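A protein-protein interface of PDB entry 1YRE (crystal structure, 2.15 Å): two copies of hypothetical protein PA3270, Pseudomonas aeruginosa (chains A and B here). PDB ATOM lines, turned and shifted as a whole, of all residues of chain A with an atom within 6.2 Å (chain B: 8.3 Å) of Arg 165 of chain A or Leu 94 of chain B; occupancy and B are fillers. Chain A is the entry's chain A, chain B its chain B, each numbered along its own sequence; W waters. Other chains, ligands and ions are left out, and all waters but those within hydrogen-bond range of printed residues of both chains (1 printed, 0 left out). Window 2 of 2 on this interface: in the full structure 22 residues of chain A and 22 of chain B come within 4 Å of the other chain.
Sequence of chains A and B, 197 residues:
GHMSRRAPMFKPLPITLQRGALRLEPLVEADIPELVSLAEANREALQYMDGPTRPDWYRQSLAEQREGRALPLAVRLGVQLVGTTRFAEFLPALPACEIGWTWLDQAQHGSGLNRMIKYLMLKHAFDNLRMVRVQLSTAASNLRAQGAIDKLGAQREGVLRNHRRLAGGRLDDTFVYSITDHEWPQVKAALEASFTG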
ATOM      1  N   TYR A  48       4.824  -1.520 -21.536  1.00  0.00           N
ATOM      2  CA  TYR A  48       5.684  -0.366 -21.189  1.00  0.00           C
ATOM      3  C   TYR A  48       7.106  -0.767 -20.780  1.00  0.00           C
ATOM      4  O   TYR A  48       7.863   0.072 -20.351  1.00  0.00           O
ATOM      5  CB  TYR A  48       5.059   0.430 -20.071  1.00  0.00           C
ATOM      6  CG  TYR A  48       3.654   0.902 -20.333  1.00  0.00           C
ATOM      7  CD1 TYR A  48       3.411   1.957 -21.196  1.00  0.00           C
ATOM      8  CD2 TYR A  48       2.580   0.303 -19.680  1.00  0.00           C
ATOM      9  CE1 TYR A  48       2.104   2.395 -21.434  1.00  0.00           C
ATOM     10  CE2 TYR A  48       1.284   0.714 -19.889  1.00  0.00           C
ATOM     11  CZ  TYR A  48       1.055   1.768 -20.754  1.00  0.00           C
ATOM     12  OH  TYR A  48      -0.220   2.166 -20.962  1.00  0.00           O
ATOM     13  N   MET A  49       7.414  -2.057 -20.891  1.00  0.00           N
ATOM     14  CA  MET A  49       8.720  -2.618 -20.587  1.00  0.00           C
ATOM     15  C   MET A  49       9.359  -3.134 -21.873  1.00  0.00           C
ATOM     16  O   MET A  49       8.684  -3.695 -22.747  1.00  0.00           O
ATOM     17  CB  MET A  49       8.608  -3.778 -19.594  1.00  0.00           C
ATOM     18  CG  MET A  49       7.927  -3.451 -18.229  1.00  0.00           C
ATOM     19  SD  MET A  49       7.938  -4.841 -17.091  1.00  0.00           S
ATOM     20  CE  MET A  49       9.647  -4.826 -16.570  1.00  0.00           C
ATOM     21  N   ASP A  50      10.672  -2.984 -21.993  1.00  0.00           N
ATOM     22  CA  ASP A  50      11.394  -3.463 -23.171  1.00  0.00           C
ATOM     23  C   ASP A  50      12.297  -4.643 -22.820  1.00  0.00           C
ATOM     24  O   ASP A  50      13.273  -4.473 -22.092  1.00  0.00           O
ATOM     25  CB  ASP A  50      12.279  -2.336 -23.698  1.00  0.00           C
ATOM     26  CG  ASP A  50      13.047  -2.734 -24.935  1.00  0.00           C
ATOM     27  OD1 ASP A  50      12.560  -3.639 -25.676  1.00  0.00           O
ATOM     28  OD2 ASP A  50      14.122  -2.107 -25.170  1.00  0.00           O
ATOM     29  N   ASN A 162      13.921  10.950 -22.993  1.00  0.00           N
ATOM     30  CA  ASN A 162      14.555  10.046 -23.975  1.00  0.00           C
ATOM     31  C   ASN A 162      15.417   8.979 -23.293  1.00  0.00           C
ATOM     32  O   ASN A 162      16.579   8.723 -23.711  1.00  0.00           O
ATOM     33  CB  ASN A 162      15.406  10.869 -24.968  1.00  0.00           C
ATOM     34  CG  ASN A 162      14.567  11.609 -26.025  1.00  0.00           C
ATOM     35  OD1 ASN A 162      13.320  11.589 -25.995  1.00  0.00           O
ATOM     36  ND2 ASN A 162      15.251  12.221 -27.001  1.00  0.00           N
ATOM     37  N   HIS A 163      14.851   8.352 -22.261  1.00  0.00           N
ATOM     38  CA  HIS A 163      15.637   7.569 -21.312  1.00  0.00           C
ATOM     39  C   HIS A 163      15.324   6.091 -21.433  1.00  0.00           C
ATOM     40  O   HIS A 163      16.096   5.264 -20.964  1.00  0.00           O
ATOM     41  CB  HIS A 163      15.433   8.048 -19.851  1.00  0.00           C
ATOM     42  CG  HIS A 163      16.302   7.337 -18.834  1.00  0.00           C
ATOM     43  ND1 HIS A 163      15.816   6.328 -18.025  1.00  0.00           N
ATOM     44  CD2 HIS A 163      17.621   7.453 -18.528  1.00  0.00           C
ATOM     45  CE1 HIS A 163      16.797   5.862 -17.251  1.00  0.00           C
ATOM     46  NE2 HIS A 163      17.898   6.534 -17.532  1.00  0.00           N
ATOM     47  N   ARG A 164      14.239   5.766 -22.129  1.00  0.00           N
ATOM     48  CA  ARG A 164      13.823   4.372 -22.300  1.00  0.00           C
ATOM     49  C   ARG A 164      13.091   4.066 -23.609  1.00  0.00           C
ATOM     50  O   ARG A 164      12.650   4.974 -24.340  1.00  0.00           O
ATOM     51  CB  ARG A 164      12.964   3.921 -21.097  1.00  0.00           C
ATOM     52  CG  ARG A 164      11.626   4.616 -21.010  1.00  0.00           C
ATOM     53  CD  ARG A 164      10.724   3.900 -20.022  1.00  0.00           C
ATOM     54  NE  ARG A 164      11.285   4.029 -18.687  1.00  0.00           N
ATOM     55  CZ  ARG A 164      11.420   3.042 -17.810  1.00  0.00           C
ATOM     56  NH1 ARG A 164      10.968   1.822 -18.090  1.00  0.00           N
ATOM     57  NH2 ARG A 164      11.996   3.294 -16.629  1.00  0.00           N
ATOM     58  N   ARG A 165      12.998   2.773 -23.903  1.00  0.00           N
ATOM     59  CA  ARG A 165      12.047   2.263 -24.887  1.00  0.00           C
ATOM     60  C   ARG A 165      10.952   1.413 -24.248  1.00  0.00           C
ATOM     61  O   ARG A 165      11.165   0.704 -23.222  1.00  0.00           O
ATOM     62  CB  ARG A 165      12.757   1.509 -25.996  1.00  0.00           C
ATOM     63  CG  ARG A 165      13.627   2.476 -26.823  1.00  0.00           C
ATOM     64  CD  ARG A 165      14.249   1.860 -28.036  1.00  0.00           C
ATOM     65  NE  ARG A 165      15.117   2.878 -28.612  1.00  0.00           N
ATOM     66  CZ  ARG A 165      14.738   3.851 -29.437  1.00  0.00           C
ATOM     67  NH1 ARG A 165      13.480   3.963 -29.850  1.00  0.00           N
ATOM     68  NH2 ARG A 165      15.641   4.732 -29.851  1.00  0.00           N
ATOM     69  N   LEU A 166       9.778   1.520 -24.873  1.00  0.00           N
ATOM     70  CA  LEU A 166       8.627   0.668 -24.594  1.00  0.00           C
ATOM     71  C   LEU A 166       8.768  -0.595 -25.435  1.00  0.00           C
ATOM     72  O   LEU A 166       9.656  -0.669 -26.302  1.00  0.00           O
ATOM     73  CB  LEU A 166       7.338   1.403 -24.925  1.00  0.00           C
ATOM     74  CG  LEU A 166       7.224   2.784 -24.247  1.00  0.00           C
ATOM     75  CD1 LEU A 166       5.923   3.478 -24.431  1.00  0.00           C
ATOM     76  CD2 LEU A 166       7.645   2.737 -22.800  1.00  0.00           C
ATOM     77  N   ALA A 167       7.908  -1.580 -25.171  1.00  0.00           N
ATOM     78  CA  ALA A 167       7.974  -2.906 -25.810  1.00  0.00           C
ATOM     79  C   ALA A 167       7.972  -2.875 -27.332  1.00  0.00           C
ATOM     80  O   ALA A 167       8.636  -3.684 -27.968  1.00  0.00           O
ATOM     81  CB  ALA A 167       6.804  -3.800 -25.297  1.00  0.00           C
ATOM     82  N   GLY A 169       9.205  -0.514 -29.096  1.00  0.00           N
ATOM     83  CA  GLY A 169      10.365   0.296 -29.509  1.00  0.00           C
ATOM     84  C   GLY A 169      10.277   1.830 -29.399  1.00  0.00           C
ATOM     85  O   GLY A 169      11.309   2.531 -29.498  1.00  0.00           O
ATOM     86  N   ARG A 170       9.069   2.349 -29.172  1.00  0.00           N
ATOM     87  CA  ARG A 170       8.869   3.767 -28.942  1.00  0.00           C
ATOM     88  C   ARG A 170       9.681   4.312 -27.734  1.00  0.00           C
ATOM     89  O   ARG A 170       9.723   3.695 -26.663  1.00  0.00           O
ATOM     90  CB  ARG A 170       7.378   4.045 -28.742  1.00  0.00           C
ATOM     91  CG  ARG A 170       7.099   5.424 -28.218  1.00  0.00           C
ATOM     92  CD  ARG A 170       5.660   5.906 -28.302  1.00  0.00           C
ATOM     93  NE  ARG A 170       5.784   7.336 -28.627  1.00  0.00           N
ATOM     94  CZ  ARG A 170       6.040   8.321 -27.752  1.00  0.00           C
ATOM     95  NH1 ARG A 170       6.143   8.073 -26.426  1.00  0.00           N
ATOM     96  NH2 ARG A 170       6.160   9.571 -28.201  1.00  0.00           N
ATOM     97  N   LEU A 171      10.279   5.481 -27.932  1.00  0.00           N
ATOM     98  CA  LEU A 171      11.051   6.186 -26.913  1.00  0.00           C
ATOM     99  C   LEU A 171      10.140   6.865 -25.874  1.00  0.00           C
ATOM    100  O   LEU A 171       9.090   7.377 -26.200  1.00  0.00           O
ATOM    101  CB  LEU A 171      11.943   7.236 -27.610  1.00  0.00           C
ATOM    102  CG  LEU A 171      13.319   7.677 -27.141  1.00  0.00           C
ATOM    103  CD1 LEU A 171      14.183   6.542 -26.777  1.00  0.00           C
ATOM    104  CD2 LEU A 171      13.963   8.497 -28.294  1.00  0.00           C
ATOM    105  N   ASP A 172      10.535   6.858 -24.607  1.00  0.00           N
ATOM    106  CA  ASP A 172       9.705   7.449 -23.592  1.00  0.00           C
ATOM    107  C   ASP A 172      10.646   8.032 -22.553  1.00  0.00           C
ATOM    108  O   ASP A 172      11.876   7.766 -22.585  1.00  0.00           O
ATOM    109  CB  ASP A 172       8.737   6.419 -22.991  1.00  0.00           C
ATOM    110  CG  ASP A 172       7.508   7.076 -22.293  1.00  0.00           C
ATOM    111  OD1 ASP A 172       7.332   8.330 -22.328  1.00  0.00           O
ATOM    112  OD2 ASP A 172       6.712   6.332 -21.681  1.00  0.00           O
ATOM    113  N   PHE B  10      25.321  -1.638 -30.904  1.00  0.00           N
ATOM    114  CA  PHE B  10      26.045  -0.612 -30.101  1.00  0.00           C
ATOM    115  C   PHE B  10      27.432  -1.064 -29.648  1.00  0.00           C
ATOM    116  O   PHE B  10      27.539  -1.868 -28.737  1.00  0.00           O
ATOM    117  CB  PHE B  10      25.226  -0.257 -28.852  1.00  0.00           C
ATOM    118  CG  PHE B  10      25.713   0.982 -28.125  1.00  0.00           C
ATOM    119  CD1 PHE B  10      25.700   2.217 -28.751  1.00  0.00           C
ATOM    120  CD2 PHE B  10      26.173   0.893 -26.822  1.00  0.00           C
ATOM    121  CE1 PHE B  10      26.156   3.350 -28.121  1.00  0.00           C
ATOM    122  CE2 PHE B  10      26.619   2.018 -26.155  1.00  0.00           C
ATOM    123  CZ  PHE B  10      26.596   3.267 -26.816  1.00  0.00           C
ATOM    124  N   GLU B  89      28.014   5.042 -18.359  1.00  0.00           N
ATOM    125  CA  GLU B  89      26.579   4.718 -18.216  1.00  0.00           C
ATOM    126  C   GLU B  89      25.876   4.610 -19.558  1.00  0.00           C
ATOM    127  O   GLU B  89      24.881   5.335 -19.826  1.00  0.00           O
ATOM    128  CB  GLU B  89      25.818   5.720 -17.311  1.00  0.00           C
ATOM    129  CG  GLU B  89      26.578   6.291 -16.192  1.00  0.00           C
ATOM    130  CD  GLU B  89      26.584   5.419 -14.942  1.00  0.00           C
ATOM    131  OE1 GLU B  89      26.149   4.237 -15.010  1.00  0.00           O
ATOM    132  OE2 GLU B  89      27.030   5.937 -13.877  1.00  0.00           O
ATOM    133  N   PHE B  90      26.376   3.690 -20.399  1.00  0.00           N
ATOM    134  CA  PHE B  90      25.774   3.445 -21.705  1.00  0.00           C
ATOM    135  C   PHE B  90      24.418   2.823 -21.560  1.00  0.00           C
ATOM    136  O   PHE B  90      24.236   1.979 -20.689  1.00  0.00           O
ATOM    137  CB  PHE B  90      26.644   2.525 -22.527  1.00  0.00           C
ATOM    138  CG  PHE B  90      28.024   3.080 -22.775  1.00  0.00           C
ATOM    139  CD1 PHE B  90      29.139   2.268 -22.692  1.00  0.00           C
ATOM    140  CD2 PHE B  90      28.198   4.416 -23.052  1.00  0.00           C
ATOM    141  CE1 PHE B  90      30.418   2.787 -22.908  1.00  0.00           C
ATOM    142  CE2 PHE B  90      29.467   4.927 -23.271  1.00  0.00           C
ATOM    143  CZ  PHE B  90      30.576   4.104 -23.207  1.00  0.00           C
ATOM    144  N   LEU B  91      23.453   3.315 -22.358  1.00  0.00           N
ATOM    145  CA  LEU B  91      22.169   2.656 -22.501  1.00  0.00           C
ATOM    146  C   LEU B  91      22.101   2.230 -23.963  1.00  0.00           C
ATOM    147  O   LEU B  91      21.642   2.993 -24.776  1.00  0.00           O
ATOM    148  CB  LEU B  91      21.012   3.612 -22.080  1.00  0.00           C
ATOM    149  CG  LEU B  91      20.983   4.193 -20.654  1.00  0.00           C
ATOM    150  CD1 LEU B  91      19.772   5.078 -20.373  1.00  0.00           C
ATOM    151  CD2 LEU B  91      21.033   3.062 -19.593  1.00  0.00           C
ATOM    152  N   PRO B  92      22.578   0.994 -24.297  1.00  0.00           N
ATOM    153  CA  PRO B  92      22.738   0.501 -25.670  1.00  0.00           C
ATOM    154  C   PRO B  92      21.434   0.493 -26.466  1.00  0.00           C
ATOM    155  O   PRO B  92      21.465   0.724 -27.683  1.00  0.00           O
ATOM    156  CB  PRO B  92      23.180  -0.953 -25.495  1.00  0.00           C
ATOM    157  CG  PRO B  92      23.617  -1.093 -24.126  1.00  0.00           C
ATOM    158  CD  PRO B  92      22.998  -0.013 -23.305  1.00  0.00           C
ATOM    159  N   ALA B  93      20.294   0.263 -25.788  1.00  0.00           N
ATOM    160  CA  ALA B  93      19.010   0.114 -26.530  1.00  0.00           C
ATOM    161  C   ALA B  93      18.519   1.424 -27.039  1.00  0.00           C
ATOM    162  O   ALA B  93      17.571   1.469 -27.818  1.00  0.00           O
ATOM    163  CB  ALA B  93      17.943  -0.547 -25.678  1.00  0.00           C
ATOM    164  N   LEU B  94      19.144   2.512 -26.578  1.00  0.00           N
ATOM    165  CA  LEU B  94      18.662   3.827 -26.934  1.00  0.00           C
ATOM    166  C   LEU B  94      19.182   4.421 -28.264  1.00  0.00           C
ATOM    167  O   LEU B  94      18.366   4.691 -29.148  1.00  0.00           O
ATOM    168  CB  LEU B  94      18.762   4.799 -25.736  1.00  0.00           C
ATOM    169  CG  LEU B  94      18.155   4.364 -24.411  1.00  0.00           C
ATOM    170  CD1 LEU B  94      17.843   5.580 -23.666  1.00  0.00           C
ATOM    171  CD2 LEU B  94      16.906   3.547 -24.518  1.00  0.00           C
ATOM    172  N   PRO B  95      20.516   4.679 -28.410  1.00  0.00           N
ATOM    173  CA  PRO B  95      21.610   4.581 -27.446  1.00  0.00           C
ATOM    174  C   PRO B  95      21.713   5.905 -26.623  1.00  0.00           C
ATOM    175  O   PRO B  95      21.236   6.928 -27.056  1.00  0.00           O
ATOM    176  CB  PRO B  95      22.828   4.373 -28.344  1.00  0.00           C
ATOM    177  CG  PRO B  95      22.469   5.135 -29.597  1.00  0.00           C
ATOM    178  CD  PRO B  95      20.992   5.160 -29.726  1.00  0.00           C
ATOM    179  N   ALA B  96      22.279   5.860 -25.429  1.00  0.00           N
ATOM    180  CA  ALA B  96      22.443   7.083 -24.613  1.00  0.00           C
ATOM    181  C   ALA B  96      23.654   6.812 -23.767  1.00  0.00           C
ATOM    182  O   ALA B  96      24.016   5.652 -23.589  1.00  0.00           O
ATOM    183  CB  ALA B  96      21.210   7.312 -23.694  1.00  0.00           C
ATOM    184  N   CYS B  97      24.219   7.870 -23.195  1.00  0.00           N
ATOM    185  CA  CYS B  97      25.289   7.743 -22.218  1.00  0.00           C
ATOM    186  C   CYS B  97      25.328   8.969 -21.265  1.00  0.00           C
ATOM    187  O   CYS B  97      24.537   9.898 -21.386  1.00  0.00           O
ATOM    188  CB  CYS B  97      26.626   7.612 -22.964  1.00  0.00           C
ATOM    189  SG  CYS B  97      27.100   9.174 -23.761  1.00  0.00           S
ATOM    190  N   LEU B 129      27.819   8.547 -32.670  1.00  0.00           N
ATOM    191  CA  LEU B 129      27.247   7.373 -31.988  1.00  0.00           C
ATOM    192  C   LEU B 129      25.736   7.354 -32.116  1.00  0.00           C
ATOM    193  O   LEU B 129      25.102   6.358 -31.726  1.00  0.00           O
ATOM    194  CB  LEU B 129      27.678   7.244 -30.514  1.00  0.00           C
ATOM    195  CG  LEU B 129      29.154   7.062 -30.253  1.00  0.00           C
ATOM    196  CD1 LEU B 129      29.524   7.163 -28.747  1.00  0.00           C
ATOM    197  CD2 LEU B 129      29.677   5.729 -30.905  1.00  0.00           C
ATOM    198  N   ARG B 130      25.181   8.453 -32.641  1.00  0.00           N
ATOM    199  CA  ARG B 130      23.750   8.567 -32.952  1.00  0.00           C
ATOM    200  C   ARG B 130      22.906   8.425 -31.663  1.00  0.00           C
ATOM    201  O   ARG B 130      21.851   7.811 -31.654  1.00  0.00           O
ATOM    202  CB  ARG B 130      23.333   7.557 -34.074  1.00  0.00           C
ATOM    203  CG  ARG B 130      24.006   7.850 -35.441  1.00  0.00           C
ATOM    204  CD  ARG B 130      23.570   6.888 -36.560  1.00  0.00           C
ATOM    205  NE  ARG B 130      22.228   7.200 -37.096  1.00  0.00           N
ATOM    206  CZ  ARG B 130      21.360   6.286 -37.540  1.00  0.00           C
ATOM    207  NH1 ARG B 130      21.664   4.982 -37.506  1.00  0.00           N
ATOM    208  NH2 ARG B 130      20.171   6.664 -38.017  1.00  0.00           N
ATOM    209  N   MET B 131      23.391   9.008 -30.564  1.00  0.00           N
ATOM    210  CA  MET B 131      22.638   8.965 -29.306  1.00  0.00           C
ATOM    211  C   MET B 131      21.431   9.887 -29.351  1.00  0.00           C
ATOM    212  O   MET B 131      21.432  10.910 -30.033  1.00  0.00           O
ATOM    213  CB  MET B 131      23.559   9.321 -28.173  1.00  0.00           C
ATOM    214  CG  MET B 131      24.481   8.114 -27.865  1.00  0.00           C
ATOM    215  SD  MET B 131      25.691   8.513 -26.693  1.00  0.00           S
ATOM    216  CE  MET B 131      26.484   6.901 -26.781  1.00  0.00           C
ATOM    217  N   VAL B 132      20.402   9.506 -28.607  1.00  0.00           N
ATOM    218  CA  VAL B 132      19.185  10.289 -28.481  1.00  0.00           C
ATOM    219  C   VAL B 132      19.166  11.134 -27.196  1.00  0.00           C
ATOM    220  O   VAL B 132      18.293  11.994 -27.028  1.00  0.00           O
ATOM    221  CB  VAL B 132      17.969   9.337 -28.540  1.00  0.00           C
ATOM    222  CG1 VAL B 132      17.995   8.556 -29.871  1.00  0.00           C
ATOM    223  CG2 VAL B 132      17.991   8.348 -27.324  1.00  0.00           C
ATOM    224  N   ARG B 133      20.140  10.896 -26.301  1.00  0.00           N
ATOM    225  CA  ARG B 133      20.197  11.569 -25.006  1.00  0.00           C
ATOM    226  C   ARG B 133      21.655  11.549 -24.546  1.00  0.00           C
ATOM    227  O   ARG B 133      22.303  10.494 -24.562  1.00  0.00           O
ATOM    228  CB  ARG B 133      19.388  10.776 -23.962  1.00  0.00           C
ATOM    229  CG  ARG B 133      19.693  11.112 -22.518  1.00  0.00           C
ATOM    230  CD  ARG B 133      18.932  10.123 -21.522  1.00  0.00           C
ATOM    231  NE  ARG B 133      19.216  10.476 -20.162  1.00  0.00           N
ATOM    232  CZ  ARG B 133      18.635  11.476 -19.509  1.00  0.00           C
ATOM    233  NH1 ARG B 133      19.027  11.765 -18.278  1.00  0.00           N
ATOM    234  NH2 ARG B 133      17.662  12.169 -20.094  1.00  0.00           N
ATOM    235  N   ASP B 181      18.718  14.641 -28.555  1.00  0.00           N
ATOM    236  CA  ASP B 181      19.182  14.781 -29.908  1.00  0.00           C
ATOM    237  C   ASP B 181      18.520  15.953 -30.602  1.00  0.00           C
ATOM    238  O   ASP B 181      19.187  16.662 -31.373  1.00  0.00           O
ATOM    239  CB  ASP B 181      19.023  13.452 -30.690  1.00  0.00           C
ATOM    240  CG  ASP B 181      17.617  12.838 -30.563  1.00  0.00           C
ATOM    241  OD1 ASP B 181      16.808  13.156 -29.642  1.00  0.00           O
ATOM    242  OD2 ASP B 181      17.320  12.025 -31.428  1.00  0.00           O
HETATM  243  O   HOH W   1      17.882   5.521 -31.780  1.00  0.00           O
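The side-chain amide nitrogen of Asn 162 of chain A is in hydrogen-bond range of the side-chain carboxylate of Asp 181 of chain B. O of Leu 94 of chain B lies within hydrogen-bond range of NH2 of Arg 165 of chain A (2.8 Å). The guanidinium group (NE) of Arg 165 of chain A is in hydrogen-bond range of the backbone carbonyl oxygen (O) of Ala 93 of chain B. The backbone carbonyl oxygen of Val 132 of chain B sits at hydrogen-bond distance from the side-chain amide nitrogen of Asn 162 of chain A, 3.1 Å away.
N of Asp 172 of chain A lies within hydrogen-bond range of O of Arg 164 of chain A, at 2.8 Å. The backbone NH (N) of Leu 91 of chain B sits at hydrogen-bond distance from the backbone carbonyl oxygen (O) of Ala 96 of chain B, 2.7 Å away. The backbone carbonyl oxygen of Pro 95 of chain B is in hydrogen-bond range of the backbone NH of Val 132 of chain B, 3.1 Å away. The backbone carbonyl oxygen of Asp 172 of chain A sits at hydrogen-bond distance from the backbone NH of His 163 of chain A, 3.0 Å away. NH1 of Arg 165 of chain A is in hydrogen-bond range of O of Gly 169 of chain A (2.6 Å). N of Asp 181 of chain B is in hydrogen-bond range of O of Val 132 of chain B, 3.1 Å away.
No position is printed for both chains.
Of chain A, only Asn 162 (3.4 Å), His 163 (3.2 Å), Arg 164 (3.9 Å) and Arg 165 (2.8 Å) come within 4 Å of Leu 94 of chain B. Printed residues of chain B within 4 Å of Asn 162 of chain A: Leu 94 (3.4 Å), Val 132 (3.1 Å), Arg 133 (3.5 Å) and Asp 181 (3.2 Å). Printed residues of chain B within 4 Å of His 163 of chain A: Leu 91, Leu 94 and Arg 133. Printed residues of chain A within 4 Å of Arg 133 of chain B: Asn 162 (3.5 Å) and His 163 (3.8 Å). Of the printed residues of chain A, Ala 93 of chain B touches Arg 165. Of the printed residues of chain A, Leu 91 of chain B touches His 163. Pro 95 of chain B touches none of the printed residues of chain A. The nearest residue of chain B that does not touch Arg 165 of chain A is Val 132 of chain B (4.5 Å). The nearest residue of chain A that does not touch Leu 94 of chain B is Leu 171 of chain A (4.6 Å).
Of the 13 printed residues of chain A, 4 touch a printed residue of chain B. Hydrophobic or aromatic side chains of chain A within 4 Å of the printed part of chain B: His 163. Along chain A the printed residues that touch a printed residue of chain B span positions 162 to 165. Among the printed residues, 10 pairs touch across the chains. Among the printed residues, no Asp or Glu carboxylate lies within 4 Å of a Lys or Arg side-chain nitrogen of the other chain.
Among the printed residues, pairs that only touch across the chains: His 163 of chain A with Leu 94 of chain B (3.2 Å), Asn 162 of chain A with Leu 94 of chain B (3.4 Å), Asn 162 of chain A with Arg 133 of chain B (3.5 Å), His 163 of chain A with Leu 91 of chain B (3.7 Å), His 163 of chain A with Arg 133 of chain B (3.8 Å) and Arg 164 of chain A with Leu 94 of chain B (3.9 Å).
Water W1 lies within hydrogen-bond range of the backbone carbonyl oxygen of Leu 94 of chain B (2.8 Å) and the guanidinium group of Arg 165 of chain A (3.1 Å).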
